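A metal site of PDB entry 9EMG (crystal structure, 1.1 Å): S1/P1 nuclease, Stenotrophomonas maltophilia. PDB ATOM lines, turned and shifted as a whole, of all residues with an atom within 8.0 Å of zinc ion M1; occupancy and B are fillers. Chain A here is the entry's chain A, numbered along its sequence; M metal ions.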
ATOM      1  N   TRP A   1      23.666  -4.453 -20.957  1.00  0.00           N
ATOM      2  CA  TRP A   1      25.057  -4.595 -20.485  1.00  0.00           C
ATOM      3  C   TRP A   1      25.106  -5.574 -19.321  1.00  0.00           C
ATOM      4  O   TRP A   1      24.104  -5.793 -18.654  1.00  0.00           O
ATOM      5  CB  TRP A   1      25.624  -3.249 -19.995  1.00  0.00           C
ATOM      6  CG  TRP A   1      25.558  -2.149 -20.999  1.00  0.00           C
ATOM      7  CD1 TRP A   1      24.606  -1.187 -21.088  1.00  0.00           C
ATOM      8  CD2 TRP A   1      26.481  -1.905 -22.069  1.00  0.00           C
ATOM      9  NE1 TRP A   1      24.875  -0.350 -22.114  1.00  0.00           N
ATOM     10  CE2 TRP A   1      26.034  -0.737 -22.735  1.00  0.00           C
ATOM     11  CE3 TRP A   1      27.680  -2.498 -22.499  1.00  0.00           C
ATOM     12  CZ2 TRP A   1      26.686  -0.222 -23.841  1.00  0.00           C
ATOM     13  CZ3 TRP A   1      28.345  -1.957 -23.575  1.00  0.00           C
ATOM     14  CH2 TRP A   1      27.860  -0.814 -24.218  1.00  0.00           C
ATOM     15  N   GLY A   2      26.296  -6.081 -19.058  1.00  0.00           N
ATOM     16  CA  GLY A   2      26.592  -6.685 -17.764  1.00  0.00           C
ATOM     17  C   GLY A   2      26.804  -5.638 -16.707  1.00  0.00           C
ATOM     18  O   GLY A   2      26.603  -4.418 -16.931  1.00  0.00           O
ATOM     19  N   HIS A   6      26.754  -1.274 -16.689  1.00  0.00           N
ATOM     20  CA  HIS A   6      25.697  -0.524 -16.000  1.00  0.00           C
ATOM     21  C   HIS A   6      26.293   0.442 -14.973  1.00  0.00           C
ATOM     22  O   HIS A   6      25.835   1.594 -14.924  1.00  0.00           O
ATOM     23  CB  HIS A   6      24.685  -1.475 -15.339  1.00  0.00           C
ATOM     24  CG  HIS A   6      23.759  -2.038 -16.344  1.00  0.00           C
ATOM     25  ND1 HIS A   6      22.842  -1.222 -16.975  1.00  0.00           N
ATOM     26  CD2 HIS A   6      23.643  -3.247 -16.912  1.00  0.00           C
ATOM     27  CE1 HIS A   6      22.216  -1.951 -17.923  1.00  0.00           C
ATOM     28  NE2 HIS A   6      22.694  -3.196 -17.894  1.00  0.00           N
ATOM     29  N   ASP A  45      18.868  -6.301 -13.263  1.00  0.00           N
ATOM     30  CA  ASP A  45      19.280  -7.624 -13.791  1.00  0.00           C
ATOM     31  C   ASP A  45      19.345  -8.704 -12.708  1.00  0.00           C
ATOM     32  O   ASP A  45      19.479  -9.881 -13.059  1.00  0.00           O
ATOM     33  CB  ASP A  45      20.633  -7.527 -14.481  1.00  0.00           C
ATOM     34  CG  ASP A  45      20.631  -6.968 -15.882  1.00  0.00           C
ATOM     35  OD1 ASP A  45      19.533  -6.811 -16.453  1.00  0.00           O
ATOM     36  OD2 ASP A  45      21.730  -6.689 -16.393  1.00  0.00           O
ATOM     37  N   HIS A  62      14.045  -4.887 -20.693  1.00  0.00           N
ATOM     38  CA  HIS A  62      15.469  -4.612 -20.953  1.00  0.00           C
ATOM     39  C   HIS A  62      15.768  -4.484 -22.447  1.00  0.00           C
ATOM     40  O   HIS A  62      16.914  -4.156 -22.796  1.00  0.00           O
ATOM     41  CB  HIS A  62      16.337  -5.675 -20.313  1.00  0.00           C
ATOM     42  CG  HIS A  62      16.214  -5.750 -18.838  1.00  0.00           C
ATOM     43  ND1 HIS A  62      17.293  -5.608 -17.992  1.00  0.00           N
ATOM     44  CD2 HIS A  62      15.135  -5.994 -18.065  1.00  0.00           C
ATOM     45  CE1 HIS A  62      16.860  -5.769 -16.742  1.00  0.00           C
ATOM     46  NE2 HIS A  62      15.529  -5.967 -16.759  1.00  0.00           N
ATOM     47  N   TYR A  63      14.800  -4.772 -23.331  1.00  0.00           N
ATOM     48  CA  TYR A  63      15.028  -4.944 -24.791  1.00  0.00           C
ATOM     49  C   TYR A  63      13.974  -4.229 -25.614  1.00  0.00           C
ATOM     50  O   TYR A  63      12.833  -4.026 -25.150  1.00  0.00           O
ATOM     51  CB  TYR A  63      14.989  -6.422 -25.216  1.00  0.00           C
ATOM     52  CG  TYR A  63      15.611  -7.370 -24.229  1.00  0.00           C
ATOM     53  CD1 TYR A  63      16.975  -7.544 -24.184  1.00  0.00           C
ATOM     54  CD2 TYR A  63      14.857  -8.030 -23.284  1.00  0.00           C
ATOM     55  CE1 TYR A  63      17.571  -8.374 -23.257  1.00  0.00           C
ATOM     56  CE2 TYR A  63      15.421  -8.859 -22.348  1.00  0.00           C
ATOM     57  CZ  TYR A  63      16.790  -9.046 -22.328  1.00  0.00           C
ATOM     58  OH  TYR A  63      17.344  -9.877 -21.392  1.00  0.00           O
ATOM     59  N   HIS A 115      19.226   1.812 -14.860  1.00  0.00           N
ATOM     60  CA  HIS A 115      19.552   0.561 -15.590  1.00  0.00           C
ATOM     61  C   HIS A 115      19.149   0.663 -17.057  1.00  0.00           C
ATOM     62  O   HIS A 115      19.898   0.309 -17.945  1.00  0.00           O
ATOM     63  CB  HIS A 115      18.849  -0.621 -14.933  1.00  0.00           C
ATOM     64  CG  HIS A 115      19.253  -1.931 -15.510  1.00  0.00           C
ATOM     65  ND1 HIS A 115      20.352  -2.616 -15.021  1.00  0.00           N
ATOM     66  CD2 HIS A 115      18.785  -2.644 -16.551  1.00  0.00           C
ATOM     67  CE1 HIS A 115      20.480  -3.744 -15.733  1.00  0.00           C
ATOM     68  NE2 HIS A 115      19.541  -3.766 -16.674  1.00  0.00           N
ATOM     69  N   ASP A 119      20.756   0.060 -20.759  1.00  0.00           N
ATOM     70  CA  ASP A 119      20.375  -1.008 -21.713  1.00  0.00           C
ATOM     71  C   ASP A 119      19.930  -0.452 -23.059  1.00  0.00           C
ATOM     72  O   ASP A 119      20.191  -1.077 -24.098  1.00  0.00           O
ATOM     73  CB  ASP A 119      19.307  -1.935 -21.141  1.00  0.00           C
ATOM     74  CG  ASP A 119      19.840  -3.099 -20.315  1.00  0.00           C
ATOM     75  OD1 ASP A 119      21.072  -3.285 -20.363  1.00  0.00           O
ATOM     76  OD2 ASP A 119      19.006  -3.739 -19.649  1.00  0.00           O
ATOM     77  N   GLN A 122      22.717  -0.153 -25.416  1.00  0.00           N
ATOM     78  CA  GLN A 122      23.427  -1.390 -25.804  1.00  0.00           C
ATOM     79  C   GLN A 122      22.880  -1.854 -27.140  1.00  0.00           C
ATOM     80  O   GLN A 122      21.713  -2.248 -27.208  1.00  0.00           O
ATOM     81  CB  GLN A 122      23.225  -2.414 -24.705  1.00  0.00           C
ATOM     82  CG  GLN A 122      23.630  -3.813 -25.120  1.00  0.00           C
ATOM     83  CD  GLN A 122      25.010  -3.900 -25.738  1.00  0.00           C
ATOM     84  OE1 GLN A 122      25.174  -4.266 -26.903  1.00  0.00           O
ATOM     85  NE2 GLN A 122      26.020  -3.559 -24.972  1.00  0.00           N
ATOM     86  N   MET A 124      22.925  -4.561 -28.810  1.00  0.00           N
ATOM     87  CA  MET A 124      22.336  -5.920 -28.825  1.00  0.00           C
ATOM     88  C   MET A 124      21.090  -6.027 -27.946  1.00  0.00           C
ATOM     89  O   MET A 124      20.464  -7.085 -27.927  1.00  0.00           O
ATOM     90  CB  MET A 124      23.368  -6.977 -28.417  1.00  0.00           C
ATOM     91  CG  MET A 124      24.473  -7.079 -29.447  1.00  0.00           C
ATOM     92  SD  MET A 124      23.938  -7.771 -31.016  1.00  0.00           S
ATOM     93  CE  MET A 124      25.101  -6.933 -32.101  1.00  0.00           C
ATOM     94  N   HIS A 125      20.698  -4.945 -27.269  1.00  0.00           N
ATOM     95  CA  HIS A 125      19.374  -4.845 -26.614  1.00  0.00           C
ATOM     96  C   HIS A 125      18.337  -4.176 -27.522  1.00  0.00           C
ATOM     97  O   HIS A 125      17.204  -4.008 -27.079  1.00  0.00           O
ATOM     98  CB  HIS A 125      19.487  -4.136 -25.264  1.00  0.00           C
ATOM     99  CG  HIS A 125      20.053  -4.995 -24.180  1.00  0.00           C
ATOM    100  ND1 HIS A 125      19.426  -5.144 -22.965  1.00  0.00           N
ATOM    101  CD2 HIS A 125      21.163  -5.799 -24.122  1.00  0.00           C
ATOM    102  CE1 HIS A 125      20.109  -6.016 -22.235  1.00  0.00           C
ATOM    103  NE2 HIS A 125      21.201  -6.405 -22.901  1.00  0.00           N
ATOM    104  N   LYS A 132      17.245 -13.409 -30.673  1.00  0.00           N
ATOM    105  CA  LYS A 132      17.313 -12.927 -29.267  1.00  0.00           C
ATOM    106  C   LYS A 132      18.477 -11.942 -29.120  1.00  0.00           C
ATOM    107  O   LYS A 132      19.290 -12.061 -28.184  1.00  0.00           O
ATOM    108  CB  LYS A 132      17.400 -14.085 -28.269  1.00  0.00           C
ATOM    109  CG  LYS A 132      16.135 -14.931 -28.160  1.00  0.00           C
ATOM    110  CD  LYS A 132      16.181 -15.889 -27.001  1.00  0.00           C
ATOM    111  CE  LYS A 132      15.055 -16.888 -26.994  1.00  0.00           C
ATOM    112  NZ  LYS A 132      15.212 -17.871 -28.080  1.00  0.00           N
ATOM    113  N   GLY A 133      18.491 -10.913 -29.964  1.00  0.00           N
ATOM    114  CA  GLY A 133      19.473  -9.837 -29.786  1.00  0.00           C
ATOM    115  C   GLY A 133      20.892 -10.352 -29.882  1.00  0.00           C
ATOM    116  O   GLY A 133      21.744  -9.932 -29.099  1.00  0.00           O
ATOM    117  N   ASN A 135      21.957 -13.307 -29.081  1.00  0.00           N
ATOM    118  CA  ASN A 135      22.275 -14.411 -28.141  1.00  0.00           C
ATOM    119  C   ASN A 135      22.428 -15.713 -28.893  1.00  0.00           C
ATOM    120  O   ASN A 135      23.262 -16.523 -28.493  1.00  0.00           O
ATOM    121  CB  ASN A 135      21.204 -14.617 -27.086  1.00  0.00           C
ATOM    122  CG  ASN A 135      21.505 -13.813 -25.857  1.00  0.00           C
ATOM    123  OD1 ASN A 135      22.444 -14.137 -25.112  1.00  0.00           O
ATOM    124  ND2 ASN A 135      20.718 -12.779 -25.668  1.00  0.00           N
ATOM    125  N   ASN A 147      28.851 -15.672 -27.250  1.00  0.00           N
ATOM    126  CA  ASN A 147      27.807 -15.323 -28.232  1.00  0.00           C
ATOM    127  C   ASN A 147      27.858 -13.807 -28.452  1.00  0.00           C
ATOM    128  O   ASN A 147      28.489 -13.090 -27.643  1.00  0.00           O
ATOM    129  CB  ASN A 147      26.430 -15.777 -27.794  1.00  0.00           C
ATOM    130  CG  ASN A 147      25.997 -15.047 -26.543  1.00  0.00           C
ATOM    131  OD1 ASN A 147      25.583 -13.899 -26.629  1.00  0.00           O
ATOM    132  ND2 ASN A 147      26.196 -15.617 -25.367  1.00  0.00           N
ATOM    133  N   HIS A 149      25.670 -11.413 -28.253  1.00  0.00           N
ATOM    134  CA  HIS A 149      25.027 -10.605 -27.206  1.00  0.00           C
ATOM    135  C   HIS A 149      25.989 -10.365 -26.044  1.00  0.00           C
ATOM    136  O   HIS A 149      26.221  -9.211 -25.644  1.00  0.00           O
ATOM    137  CB  HIS A 149      23.707 -11.240 -26.798  1.00  0.00           C
ATOM    138  CG  HIS A 149      22.931 -10.359 -25.882  1.00  0.00           C
ATOM    139  ND1 HIS A 149      21.882  -9.577 -26.340  1.00  0.00           N
ATOM    140  CD2 HIS A 149      23.082 -10.069 -24.560  1.00  0.00           C
ATOM    141  CE1 HIS A 149      21.422  -8.865 -25.304  1.00  0.00           C
ATOM    142  NE2 HIS A 149      22.113  -9.130 -24.207  1.00  0.00           N
ATOM    143  N   SER A 150      26.523 -11.447 -25.506  1.00  0.00           N
ATOM    144  CA  SER A 150      27.454 -11.362 -24.381  1.00  0.00           C
ATOM    145  C   SER A 150      28.719 -10.595 -24.773  1.00  0.00           C
ATOM    146  O   SER A 150      29.284  -9.868 -23.932  1.00  0.00           O
ATOM    147  CB  SER A 150      27.820 -12.738 -23.863  1.00  0.00           C
ATOM    148  OG  SER A 150      26.678 -13.364 -23.320  1.00  0.00           O
ATOM    149  N   TRP A 152      28.996  -8.068 -26.659  1.00  0.00           N
ATOM    150  CA  TRP A 152      28.674  -6.623 -26.570  1.00  0.00           C
ATOM    151  C   TRP A 152      28.329  -6.247 -25.128  1.00  0.00           C
ATOM    152  O   TRP A 152      28.677  -5.114 -24.719  1.00  0.00           O
ATOM    153  CB  TRP A 152      27.594  -6.287 -27.568  1.00  0.00           C
ATOM    154  CG  TRP A 152      28.148  -6.059 -28.929  1.00  0.00           C
ATOM    155  CD1 TRP A 152      28.505  -6.995 -29.847  1.00  0.00           C
ATOM    156  CD2 TRP A 152      28.532  -4.805 -29.474  1.00  0.00           C
ATOM    157  NE1 TRP A 152      29.092  -6.416 -30.926  1.00  0.00           N
ATOM    158  CE2 TRP A 152      29.113  -5.056 -30.734  1.00  0.00           C
ATOM    159  CE3 TRP A 152      28.465  -3.484 -29.025  1.00  0.00           C
ATOM    160  CZ2 TRP A 152      29.616  -4.042 -31.543  1.00  0.00           C
ATOM    161  CZ3 TRP A 152      28.990  -2.493 -29.809  1.00  0.00           C
ATOM    162  CH2 TRP A 152      29.542  -2.752 -31.063  1.00  0.00           C
ATOM    163  N   ASP A 153      27.632  -7.064 -24.373  1.00  0.00           N
ATOM    164  CA  ASP A 153      27.288  -6.726 -22.984  1.00  0.00           C
ATOM    165  C   ASP A 153      28.539  -6.590 -22.102  1.00  0.00           C
ATOM    166  O   ASP A 153      28.544  -5.740 -21.174  1.00  0.00           O
ATOM    167  CB  ASP A 153      26.339  -7.719 -22.354  1.00  0.00           C
ATOM    168  CG  ASP A 153      24.849  -7.455 -22.544  1.00  0.00           C
ATOM    169  OD1 ASP A 153      24.474  -6.444 -23.127  1.00  0.00           O
ATOM    170  OD2 ASP A 153      24.095  -8.293 -22.016  1.00  0.00           O
ATOM    171  N   SER A 154      29.505  -7.477 -22.304  1.00  0.00           N
ATOM    172  CA  SER A 154      30.656  -7.540 -21.390  1.00  0.00           C
ATOM    173  C   SER A 154      31.950  -8.043 -22.029  1.00  0.00           C
ATOM    174  O   SER A 154      33.002  -7.679 -21.536  1.00  0.00           O
ATOM    175  CB  SER A 154      30.382  -8.337 -20.175  1.00  0.00           C
ATOM    176  OG  SER A 154      30.058  -9.648 -20.500  1.00  0.00           O
HETATM  177 ZN    ZN M   1      22.196  -8.114 -22.467  1.00  0.00          ZN
HETATM  178 ZN    ZN M   2      22.308  -4.607 -19.325  1.00  0.00          ZN
HETATM  179 ZN    ZN M   3      19.288  -5.205 -18.170  1.00  0.00          ZN
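N of His 149 lies within hydrogen-bond range of OD1 of Asn 147 (3.0 Å).
The side-chain carboxylate (OD1) of Asp 153 sits close to the backbone NH (N) of Trp 1, at 3.1 Å.
A ring nitrogen (ND1) of His 125 lies within hydrogen-bond range of the backbone carbonyl oxygen of His 62 (2.7 Å).
O of Gly 133 is in hydrogen-bond range of ND1 of His 149.
A ring nitrogen (ND1) of His 149 lies close to the side-chain amide nitrogen (ND2) of Asn 135 (3.5 Å).
The backbone carbonyl oxygen of Asp 153 is in hydrogen-bond range of the backbone NH of Gly 2.
A ring nitrogen (ND1) of His 149 is in hydrogen-bond range of the backbone carbonyl oxygen of Met 124.
Three residues have an atom within 4 Å of zinc ion M1: His 125, His 149 and Asp 153.
The nearest printed residue that does not touch zinc ion M1 is Trp 1 (4.2 Å).
OD2 of Asp 153 binds zinc ion M1.
NE2 of His 149 binds zinc ion M1 (2.0 Å).
Zinc ion M1 is bound by a ring nitrogen (NE2) of His 125 (2.0 Å).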
